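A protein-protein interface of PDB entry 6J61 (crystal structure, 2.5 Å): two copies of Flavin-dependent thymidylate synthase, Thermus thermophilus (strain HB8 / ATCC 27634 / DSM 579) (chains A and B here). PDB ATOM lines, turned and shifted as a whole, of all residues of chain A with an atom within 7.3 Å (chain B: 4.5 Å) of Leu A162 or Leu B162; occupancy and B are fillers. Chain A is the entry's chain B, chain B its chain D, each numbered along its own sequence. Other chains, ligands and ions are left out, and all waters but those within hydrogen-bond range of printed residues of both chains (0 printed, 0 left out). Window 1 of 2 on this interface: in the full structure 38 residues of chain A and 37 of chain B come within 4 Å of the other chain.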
ATOM      1  N   ALA A  72       2.382  -1.966 -12.286  1.00  0.00           N
ATOM      2  CA  ALA A  72       1.068  -2.034 -12.905  1.00  0.00           C
ATOM      3  C   ALA A  72       1.225  -2.354 -14.375  1.00  0.00           C
ATOM      4  O   ALA A  72       2.317  -2.217 -14.943  1.00  0.00           O
ATOM      5  CB  ALA A  72       0.343  -0.691 -12.750  1.00  0.00           C
ATOM      6  N   PRO A  73       0.139  -2.816 -15.009  1.00  0.00           N
ATOM      7  CA  PRO A  73       0.216  -3.133 -16.436  1.00  0.00           C
ATOM      8  C   PRO A  73       0.234  -1.821 -17.238  1.00  0.00           C
ATOM      9  O   PRO A  73      -0.495  -0.876 -16.914  1.00  0.00           O
ATOM     10  CB  PRO A  73      -1.042  -3.970 -16.669  1.00  0.00           C
ATOM     11  CG  PRO A  73      -1.995  -3.444 -15.637  1.00  0.00           C
ATOM     12  CD  PRO A  73      -1.119  -3.313 -14.425  1.00  0.00           C
ATOM     13  N   ILE A  74       1.075  -1.764 -18.268  1.00  0.00           N
ATOM     14  CA  ILE A  74       1.197  -0.575 -19.101  1.00  0.00           C
ATOM     15  C   ILE A  74      -0.105   0.176 -19.360  1.00  0.00           C
ATOM     16  O   ILE A  74      -0.177   1.382 -19.110  1.00  0.00           O
ATOM     17  CB  ILE A  74       1.843  -0.906 -20.462  1.00  0.00           C
ATOM     18  CG1 ILE A  74       3.326  -1.225 -20.266  1.00  0.00           C
ATOM     19  CG2 ILE A  74       1.672   0.258 -21.423  1.00  0.00           C
ATOM     20  CD1 ILE A  74       4.029  -1.681 -21.520  1.00  0.00           C
ATOM     21  N   PHE A  75      -1.133  -0.519 -19.845  1.00  0.00           N
ATOM     22  CA  PHE A  75      -2.394   0.156 -20.149  1.00  0.00           C
ATOM     23  C   PHE A  75      -3.000   0.890 -18.952  1.00  0.00           C
ATOM     24  O   PHE A  75      -3.826   1.788 -19.115  1.00  0.00           O
ATOM     25  CB  PHE A  75      -3.406  -0.828 -20.781  1.00  0.00           C
ATOM     26  CG  PHE A  75      -4.116  -1.716 -19.797  1.00  0.00           C
ATOM     27  CD1 PHE A  75      -5.241  -1.259 -19.111  1.00  0.00           C
ATOM     28  CD2 PHE A  75      -3.670  -3.014 -19.567  1.00  0.00           C
ATOM     29  CE1 PHE A  75      -5.916  -2.084 -18.205  1.00  0.00           C
ATOM     30  CE2 PHE A  75      -4.334  -3.845 -18.666  1.00  0.00           C
ATOM     31  CZ  PHE A  75      -5.462  -3.379 -17.983  1.00  0.00           C
ATOM     32  N   VAL A  76      -2.581   0.516 -17.752  1.00  0.00           N
ATOM     33  CA  VAL A  76      -3.069   1.173 -16.550  1.00  0.00           C
ATOM     34  C   VAL A  76      -2.205   2.392 -16.272  1.00  0.00           C
ATOM     35  O   VAL A  76      -2.687   3.407 -15.777  1.00  0.00           O
ATOM     36  CB  VAL A  76      -3.023   0.219 -15.341  1.00  0.00           C
ATOM     37  CG1 VAL A  76      -3.104   1.001 -14.036  1.00  0.00           C
ATOM     38  CG2 VAL A  76      -4.197  -0.756 -15.424  1.00  0.00           C
ATOM     39  N   ALA A  77      -0.926   2.286 -16.612  1.00  0.00           N
ATOM     40  CA  ALA A  77       0.025   3.369 -16.411  1.00  0.00           C
ATOM     41  C   ALA A  77      -0.246   4.534 -17.364  1.00  0.00           C
ATOM     42  O   ALA A  77       0.027   5.683 -17.032  1.00  0.00           O
ATOM     43  CB  ALA A  77       1.452   2.854 -16.600  1.00  0.00           C
ATOM     44  N   ARG A  78      -0.776   4.236 -18.546  1.00  0.00           N
ATOM     45  CA  ARG A  78      -1.077   5.278 -19.514  1.00  0.00           C
ATOM     46  C   ARG A  78      -2.170   6.181 -18.986  1.00  0.00           C
ATOM     47  O   ARG A  78      -2.183   7.383 -19.250  1.00  0.00           O
ATOM     48  CB  ARG A  78      -1.530   4.683 -20.843  1.00  0.00           C
ATOM     49  CG  ARG A  78      -0.441   3.980 -21.613  1.00  0.00           C
ATOM     50  CD  ARG A  78      -0.758   4.054 -23.089  1.00  0.00           C
ATOM     51  NE  ARG A  78      -0.568   5.410 -23.605  1.00  0.00           N
ATOM     52  CZ  ARG A  78      -1.270   5.946 -24.598  1.00  0.00           C
ATOM     53  NH1 ARG A  78      -2.233   5.254 -25.200  1.00  0.00           N
ATOM     54  NH2 ARG A  78      -0.996   7.176 -25.003  1.00  0.00           N
ATOM     55  N   LEU A  98      12.479  -6.686 -20.499  1.00  0.00           N
ATOM     56  CA  LEU A  98      11.238  -6.818 -19.751  1.00  0.00           C
ATOM     57  C   LEU A  98      10.852  -8.235 -19.312  1.00  0.00           C
ATOM     58  O   LEU A  98      10.808  -9.168 -20.116  1.00  0.00           O
ATOM     59  CB  LEU A  98      10.111  -6.183 -20.573  1.00  0.00           C
ATOM     60  CG  LEU A  98      10.373  -4.704 -20.895  1.00  0.00           C
ATOM     61  CD1 LEU A  98       9.451  -4.210 -22.003  1.00  0.00           C
ATOM     62  CD2 LEU A  98      10.190  -3.885 -19.630  1.00  0.00           C
ATOM     63  N   PHE A 102       2.319 -10.560 -17.240  1.00  0.00           N
ATOM     64  CA  PHE A 102       1.237  -9.779 -17.818  1.00  0.00           C
ATOM     65  C   PHE A 102       0.052  -9.732 -16.883  1.00  0.00           C
ATOM     66  O   PHE A 102      -0.016 -10.475 -15.907  1.00  0.00           O
ATOM     67  CB  PHE A 102       0.779 -10.380 -19.151  1.00  0.00           C
ATOM     68  CG  PHE A 102       1.894 -10.656 -20.114  1.00  0.00           C
ATOM     69  CD1 PHE A 102       2.804 -11.675 -19.870  1.00  0.00           C
ATOM     70  CD2 PHE A 102       2.023  -9.907 -21.278  1.00  0.00           C
ATOM     71  CE1 PHE A 102       3.824 -11.945 -20.769  1.00  0.00           C
ATOM     72  CE2 PHE A 102       3.043 -10.170 -22.187  1.00  0.00           C
ATOM     73  CZ  PHE A 102       3.943 -11.190 -21.933  1.00  0.00           C
ATOM     74  N   TYR A 103      -0.884  -8.846 -17.188  1.00  0.00           N
ATOM     75  CA  TYR A 103      -2.081  -8.727 -16.391  1.00  0.00           C
ATOM     76  C   TYR A 103      -3.091  -9.754 -16.869  1.00  0.00           C
ATOM     77  O   TYR A 103      -3.733  -9.578 -17.909  1.00  0.00           O
ATOM     78  CB  TYR A 103      -2.688  -7.339 -16.520  1.00  0.00           C
ATOM     79  CG  TYR A 103      -4.051  -7.242 -15.884  1.00  0.00           C
ATOM     80  CD1 TYR A 103      -4.248  -7.618 -14.555  1.00  0.00           C
ATOM     81  CD2 TYR A 103      -5.145  -6.769 -16.605  1.00  0.00           C
ATOM     82  CE1 TYR A 103      -5.504  -7.523 -13.955  1.00  0.00           C
ATOM     83  CE2 TYR A 103      -6.408  -6.671 -16.015  1.00  0.00           C
ATOM     84  CZ  TYR A 103      -6.575  -7.049 -14.691  1.00  0.00           C
ATOM     85  OH  TYR A 103      -7.808  -6.951 -14.107  1.00  0.00           O
ATOM     86  N   ALA A 156      12.220  -4.394 -30.104  1.00  0.00           N
ATOM     87  CA  ALA A 156      11.755  -5.723 -29.759  1.00  0.00           C
ATOM     88  C   ALA A 156      10.491  -5.703 -28.901  1.00  0.00           C
ATOM     89  O   ALA A 156       9.507  -6.378 -29.222  1.00  0.00           O
ATOM     90  CB  ALA A 156      12.860  -6.484 -29.047  1.00  0.00           C
ATOM     91  N   ARG A 157      10.519  -4.940 -27.809  1.00  0.00           N
ATOM     92  CA  ARG A 157       9.368  -4.847 -26.906  1.00  0.00           C
ATOM     93  C   ARG A 157       8.142  -4.334 -27.643  1.00  0.00           C
ATOM     94  O   ARG A 157       7.023  -4.362 -27.139  1.00  0.00           O
ATOM     95  CB  ARG A 157       9.695  -3.936 -25.715  1.00  0.00           C
ATOM     96  CG  ARG A 157      10.349  -2.593 -26.072  1.00  0.00           C
ATOM     97  CD  ARG A 157       9.420  -1.678 -26.864  1.00  0.00           C
ATOM     98  NE  ARG A 157      10.019  -0.363 -27.078  1.00  0.00           N
ATOM     99  CZ  ARG A 157      10.147   0.571 -26.139  1.00  0.00           C
ATOM    100  NH1 ARG A 157       9.711   0.350 -24.901  1.00  0.00           N
ATOM    101  NH2 ARG A 157      10.736   1.721 -26.435  1.00  0.00           N
ATOM    102  N   MET A 158       8.377  -3.863 -28.855  1.00  0.00           N
ATOM    103  CA  MET A 158       7.326  -3.340 -29.702  1.00  0.00           C
ATOM    104  C   MET A 158       6.148  -4.323 -29.817  1.00  0.00           C
ATOM    105  O   MET A 158       4.982  -3.920 -29.758  1.00  0.00           O
ATOM    106  CB  MET A 158       7.926  -3.050 -31.078  1.00  0.00           C
ATOM    107  CG  MET A 158       7.043  -2.309 -32.036  1.00  0.00           C
ATOM    108  SD  MET A 158       7.834  -2.169 -33.643  1.00  0.00           S
ATOM    109  CE  MET A 158       9.275  -1.117 -33.240  1.00  0.00           C
ATOM    110  N   VAL A 159       6.463  -5.612 -29.962  1.00  0.00           N
ATOM    111  CA  VAL A 159       5.454  -6.666 -30.110  1.00  0.00           C
ATOM    112  C   VAL A 159       4.772  -7.114 -28.825  1.00  0.00           C
ATOM    113  O   VAL A 159       3.943  -8.019 -28.853  1.00  0.00           O
ATOM    114  CB  VAL A 159       6.059  -7.933 -30.740  1.00  0.00           C
ATOM    115  CG1 VAL A 159       6.812  -7.584 -32.020  1.00  0.00           C
ATOM    116  CG2 VAL A 159       6.973  -8.618 -29.734  1.00  0.00           C
ATOM    117  N   LEU A 160       5.126  -6.499 -27.701  1.00  0.00           N
ATOM    118  CA  LEU A 160       4.534  -6.867 -26.422  1.00  0.00           C
ATOM    119  C   LEU A 160       3.147  -6.258 -26.269  1.00  0.00           C
ATOM    120  O   LEU A 160       2.919  -5.090 -26.600  1.00  0.00           O
ATOM    121  CB  LEU A 160       5.452  -6.432 -25.271  1.00  0.00           C
ATOM    122  CG  LEU A 160       6.878  -7.014 -25.345  1.00  0.00           C
ATOM    123  CD1 LEU A 160       7.654  -6.693 -24.067  1.00  0.00           C
ATOM    124  CD2 LEU A 160       6.815  -8.535 -25.552  1.00  0.00           C
ATOM    125  N   PRO A 161       2.195  -7.046 -25.756  1.00  0.00           N
ATOM    126  CA  PRO A 161       0.823  -6.575 -25.567  1.00  0.00           C
ATOM    127  C   PRO A 161       0.728  -5.464 -24.540  1.00  0.00           C
ATOM    128  O   PRO A 161       1.628  -5.285 -23.720  1.00  0.00           O
ATOM    129  CB  PRO A 161       0.097  -7.830 -25.117  1.00  0.00           C
ATOM    130  CG  PRO A 161       1.133  -8.483 -24.268  1.00  0.00           C
ATOM    131  CD  PRO A 161       2.383  -8.360 -25.121  1.00  0.00           C
ATOM    132  N   LEU A 162      -0.386  -4.742 -24.583  1.00  0.00           N
ATOM    133  CA  LEU A 162      -0.643  -3.629 -23.681  1.00  0.00           C
ATOM    134  C   LEU A 162      -0.893  -4.060 -22.225  1.00  0.00           C
ATOM    135  O   LEU A 162      -0.969  -3.218 -21.327  1.00  0.00           O
ATOM    136  CB  LEU A 162      -1.844  -2.827 -24.199  1.00  0.00           C
ATOM    137  CG  LEU A 162      -1.742  -1.300 -24.207  1.00  0.00           C
ATOM    138  CD1 LEU A 162      -0.620  -0.836 -25.125  1.00  0.00           C
ATOM    139  CD2 LEU A 162      -3.059  -0.732 -24.667  1.00  0.00           C
ATOM    140  N   ASN A 163      -1.026  -5.360 -21.988  1.00  0.00           N
ATOM    141  CA  ASN A 163      -1.255  -5.830 -20.630  1.00  0.00           C
ATOM    142  C   ASN A 163       0.059  -6.229 -19.944  1.00  0.00           C
ATOM    143  O   ASN A 163       0.065  -6.715 -18.811  1.00  0.00           O
ATOM    144  CB  ASN A 163      -2.258  -6.988 -20.633  1.00  0.00           C
ATOM    145  CG  ASN A 163      -1.749  -8.204 -21.382  1.00  0.00           C
ATOM    146  OD1 ASN A 163      -1.177  -8.089 -22.468  1.00  0.00           O
ATOM    147  ND2 ASN A 163      -1.971  -9.381 -20.808  1.00  0.00           N
ATOM    148  N   LEU A 164       1.175  -6.010 -20.634  1.00  0.00           N
ATOM    149  CA  LEU A 164       2.488  -6.312 -20.073  1.00  0.00           C
ATOM    150  C   LEU A 164       2.642  -5.478 -18.805  1.00  0.00           C
ATOM    151  O   LEU A 164       2.076  -4.394 -18.702  1.00  0.00           O
ATOM    152  CB  LEU A 164       3.588  -5.940 -21.069  1.00  0.00           C
ATOM    153  CG  LEU A 164       5.033  -6.103 -20.590  1.00  0.00           C
ATOM    154  CD1 LEU A 164       5.373  -7.578 -20.411  1.00  0.00           C
ATOM    155  CD2 LEU A 164       5.960  -5.479 -21.600  1.00  0.00           C
ATOM    156  N   TYR A 165       3.397  -5.976 -17.836  1.00  0.00           N
ATOM    157  CA  TYR A 165       3.576  -5.229 -16.597  1.00  0.00           C
ATOM    158  C   TYR A 165       4.766  -4.285 -16.683  1.00  0.00           C
ATOM    159  O   TYR A 165       5.768  -4.576 -17.345  1.00  0.00           O
ATOM    160  CB  TYR A 165       3.777  -6.185 -15.420  1.00  0.00           C
ATOM    161  CG  TYR A 165       2.519  -6.511 -14.658  1.00  0.00           C
ATOM    162  CD1 TYR A 165       1.989  -5.610 -13.734  1.00  0.00           C
ATOM    163  CD2 TYR A 165       1.869  -7.734 -14.842  1.00  0.00           C
ATOM    164  CE1 TYR A 165       0.841  -5.917 -13.000  1.00  0.00           C
ATOM    165  CE2 TYR A 165       0.719  -8.055 -14.117  1.00  0.00           C
ATOM    166  CZ  TYR A 165       0.210  -7.144 -13.195  1.00  0.00           C
ATOM    167  OH  TYR A 165      -0.917  -7.465 -12.467  1.00  0.00           O
ATOM    168  N   PRO B  73       2.728   5.471 -33.206  1.00  0.00           N
ATOM    169  CA  PRO B  73       2.603   4.214 -32.464  1.00  0.00           C
ATOM    170  C   PRO B  73       2.541   4.475 -30.958  1.00  0.00           C
ATOM    171  O   PRO B  73       3.227   5.366 -30.440  1.00  0.00           O
ATOM    172  CB  PRO B  73       3.867   3.445 -32.858  1.00  0.00           C
ATOM    173  CG  PRO B  73       4.296   4.084 -34.155  1.00  0.00           C
ATOM    174  CD  PRO B  73       4.017   5.538 -33.910  1.00  0.00           C
ATOM    175  N   ILE B  74       1.714   3.697 -30.264  1.00  0.00           N
ATOM    176  CA  ILE B  74       1.571   3.839 -28.826  1.00  0.00           C
ATOM    177  C   ILE B  74       2.924   3.981 -28.147  1.00  0.00           C
ATOM    178  O   ILE B  74       3.133   4.913 -27.379  1.00  0.00           O
ATOM    179  CB  ILE B  74       0.833   2.629 -28.193  1.00  0.00           C
ATOM    180  CG1 ILE B  74      -0.644   2.641 -28.596  1.00  0.00           C
ATOM    181  CG2 ILE B  74       0.960   2.675 -26.675  1.00  0.00           C
ATOM    182  CD1 ILE B  74      -1.503   1.665 -27.823  1.00  0.00           C
ATOM    183  N   PHE B  75       3.854   3.074 -28.428  1.00  0.00           N
ATOM    184  CA  PHE B  75       5.142   3.176 -27.768  1.00  0.00           C
ATOM    185  C   PHE B  75       5.759   4.557 -27.976  1.00  0.00           C
ATOM    186  O   PHE B  75       6.336   5.127 -27.053  1.00  0.00           O
ATOM    187  CB  PHE B  75       6.087   2.012 -28.180  1.00  0.00           C
ATOM    188  CG  PHE B  75       6.700   2.134 -29.555  1.00  0.00           C
ATOM    189  CD1 PHE B  75       7.832   2.922 -29.769  1.00  0.00           C
ATOM    190  CD2 PHE B  75       6.178   1.414 -30.629  1.00  0.00           C
ATOM    191  CE1 PHE B  75       8.442   2.989 -31.039  1.00  0.00           C
ATOM    192  CE2 PHE B  75       6.779   1.474 -31.906  1.00  0.00           C
ATOM    193  CZ  PHE B  75       7.914   2.264 -32.107  1.00  0.00           C
ATOM    194  N   ARG B 157      -8.971  -4.331 -25.550  1.00  0.00           N
ATOM    195  CA  ARG B 157      -7.816  -3.693 -26.166  1.00  0.00           C
ATOM    196  C   ARG B 157      -6.482  -4.003 -25.499  1.00  0.00           C
ATOM    197  O   ARG B 157      -5.428  -3.703 -26.062  1.00  0.00           O
ATOM    198  CB  ARG B 157      -8.019  -2.171 -26.236  1.00  0.00           C
ATOM    199  CG  ARG B 157      -8.260  -1.465 -24.891  1.00  0.00           C
ATOM    200  CD  ARG B 157      -6.978  -1.146 -24.116  1.00  0.00           C
ATOM    201  NE  ARG B 157      -7.286  -0.549 -22.813  1.00  0.00           N
ATOM    202  CZ  ARG B 157      -7.609   0.729 -22.611  1.00  0.00           C
ATOM    203  NH1 ARG B 157      -7.658   1.578 -23.628  1.00  0.00           N
ATOM    204  NH2 ARG B 157      -7.922   1.153 -21.389  1.00  0.00           N
ATOM    205  N   MET B 158      -6.520  -4.624 -24.322  1.00  0.00           N
ATOM    206  CA  MET B 158      -5.287  -4.935 -23.606  1.00  0.00           C
ATOM    207  C   MET B 158      -4.373  -5.978 -24.253  1.00  0.00           C
ATOM    208  O   MET B 158      -3.231  -6.149 -23.814  1.00  0.00           O
ATOM    209  CB  MET B 158      -5.597  -5.382 -22.181  1.00  0.00           C
ATOM    210  CG  MET B 158      -6.118  -6.794 -22.072  1.00  0.00           C
ATOM    211  SD  MET B 158      -6.063  -7.335 -20.363  1.00  0.00           S
ATOM    212  CE  MET B 158      -7.516  -6.477 -19.687  1.00  0.00           C
ATOM    213  N   LEU B 160      -3.489  -5.889 -27.481  1.00  0.00           N
ATOM    214  CA  LEU B 160      -2.868  -5.294 -28.662  1.00  0.00           C
ATOM    215  C   LEU B 160      -1.434  -4.834 -28.387  1.00  0.00           C
ATOM    216  O   LEU B 160      -1.114  -4.378 -27.290  1.00  0.00           O
ATOM    217  CB  LEU B 160      -3.714  -4.129 -29.157  1.00  0.00           C
ATOM    218  CG  LEU B 160      -5.072  -4.560 -29.708  1.00  0.00           C
ATOM    219  CD1 LEU B 160      -5.924  -3.332 -30.024  1.00  0.00           C
ATOM    220  CD2 LEU B 160      -4.858  -5.420 -30.951  1.00  0.00           C
ATOM    221  N   PRO B 161      -0.551  -4.953 -29.391  1.00  0.00           N
ATOM    222  CA  PRO B 161       0.858  -4.567 -29.279  1.00  0.00           C
ATOM    223  C   PRO B 161       1.153  -3.071 -29.257  1.00  0.00           C
ATOM    224  O   PRO B 161       0.484  -2.276 -29.924  1.00  0.00           O
ATOM    225  CB  PRO B 161       1.495  -5.267 -30.474  1.00  0.00           C
ATOM    226  CG  PRO B 161       0.424  -5.211 -31.495  1.00  0.00           C
ATOM    227  CD  PRO B 161      -0.830  -5.546 -30.713  1.00  0.00           C
ATOM    228  N   LEU B 162       2.174  -2.703 -28.488  1.00  0.00           N
ATOM    229  CA  LEU B 162       2.595  -1.314 -28.350  1.00  0.00           C
ATOM    230  C   LEU B 162       2.830  -0.611 -29.682  1.00  0.00           C
ATOM    231  O   LEU B 162       2.874   0.617 -29.725  1.00  0.00           O
ATOM    232  CB  LEU B 162       3.889  -1.224 -27.531  1.00  0.00           C
ATOM    233  CG  LEU B 162       3.909  -1.715 -26.085  1.00  0.00           C
ATOM    234  CD1 LEU B 162       5.341  -1.671 -25.559  1.00  0.00           C
ATOM    235  CD2 LEU B 162       2.976  -0.855 -25.232  1.00  0.00           C
ATOM    236  N   ASN B 163       2.996  -1.370 -30.763  1.00  0.00           N
ATOM    237  CA  ASN B 163       3.236  -0.743 -32.052  1.00  0.00           C
ATOM    238  C   ASN B 163       1.944  -0.434 -32.793  1.00  0.00           C
ATOM    239  O   ASN B 163       1.946  -0.169 -34.002  1.00  0.00           O
ATOM    240  CB  ASN B 163       4.166  -1.607 -32.904  1.00  0.00           C
ATOM    241  CG  ASN B 163       3.464  -2.778 -33.565  1.00  0.00           C
ATOM    242  OD1 ASN B 163       2.674  -3.500 -32.945  1.00  0.00           O
ATOM    243  ND2 ASN B 163       3.772  -2.985 -34.837  1.00  0.00           N
ATOM    244  N   LEU B 164       0.840  -0.469 -32.047  1.00  0.00           N
ATOM    245  CA  LEU B 164      -0.481  -0.152 -32.573  1.00  0.00           C
ATOM    246  C   LEU B 164      -0.530   1.375 -32.709  1.00  0.00           C
ATOM    247  O   LEU B 164      -0.037   2.108 -31.834  1.00  0.00           O
ATOM    248  CB  LEU B 164      -1.567  -0.607 -31.591  1.00  0.00           C
ATOM    249  CG  LEU B 164      -3.028  -0.216 -31.882  1.00  0.00           C
ATOM    250  CD1 LEU B 164      -3.635  -1.149 -32.937  1.00  0.00           C
ATOM    251  CD2 LEU B 164      -3.844  -0.285 -30.595  1.00  0.00           C
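The backbone NH of Leu B162 sits at hydrogen-bond distance from the backbone carbonyl oxygen of Met A158 (3.3 Å). N of Asn A163 is in hydrogen-bond range of O of Met B158. The backbone NH (N) of Leu A162 sits at hydrogen-bond distance from the backbone carbonyl oxygen (O) of Leu B160 (2.8 Å). The backbone carbonyl oxygen of Met A158 is in hydrogen-bond range of the backbone NH of Asn B163 (3.4 Å). The backbone NH of Leu A162 is in hydrogen-bond range of the backbone carbonyl oxygen of Met B158, at 3.3 Å. The backbone carbonyl oxygen of Leu A160 sits at hydrogen-bond distance from the backbone NH of Leu B162, 3.1 Å away.
The backbone NH (N) of Ile A74 sits at hydrogen-bond distance from the backbone carbonyl oxygen (O) of Leu A164 (2.8 Å). O of Leu A162 lies within hydrogen-bond range of N of Phe A75, 3.1 Å away. N of Ile B74 sits close to O of Leu B162 (3.3 Å). O of Leu B164 is in hydrogen-bond range of N of Ile B74, 2.8 Å away. The backbone NH of Tyr A103 lies within hydrogen-bond range of the backbone carbonyl oxygen of Asn A163. The backbone NH (N) of Phe B75 lies within hydrogen-bond range of the backbone carbonyl oxygen (O) of Leu B162, at 2.9 Å.
Among the printed residues, pairs that only touch across the chains: Pro A161 with Leu B160 (3.4 Å), Leu A160 with Pro B161 (3.4 Å), Arg A157 with Leu B162 (3.5 Å), Leu A162 with Leu B162 (3.6 Å), Leu A162 with Ile B74 (3.8 Å), Met A158 with Phe B75 (3.8 Å), Met A158 with Pro B161 (3.8 Å), Tyr A103 with Met B158 (3.8 Å), Ile A74 with Leu B162 (3.9 Å), Pro A161 with Met B158 (3.9 Å) and Leu A162 with Arg B157 (3.98 Å).
Leu A162 touches five residues of chain B. Leu B162 touches five residues of chain A. Of the printed residues of chain A, Pro B161 touches Met A158 (3.8 Å) and Leu A160 (3.4 Å). Printed residues of chain A within 4 Å of Met B158: Tyr A103, Pro A161, Leu A162 and Asn A163. Of the printed residues of chain A, Arg B157 touches Leu A162. Val A76 touches none of the printed residues of chain B. The nearest printed residue of chain A that does not touch Asn B163 is Val A159 (5.1 Å).
Hydrophobic or aromatic side chains of chain B within 4 Å of the printed part of chain A: Ile B74, Phe B75, Met B158, Pro B161 and Leu B162. Of the 20 printed residues of chain A, 8 touch a printed residue of chain B. Among the printed residues, 17 pairs touch across the chains.
Ile A74 touches Leu B162, and with the chains exchanged Leu A162 touches Ile B74. Arg A157 touches Leu B162, and with the chains exchanged Leu A162 touches Arg B157. Met A158 touches Pro B161, and with the chains exchanged Pro A161 touches Met B158. Leu A160 touches Pro B161, and with the chains exchanged Pro A161 touches Leu B160. Of the 17 pairs that touch across the chains among the printed residues, 15 have their exchanged pair printed and touching as well.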
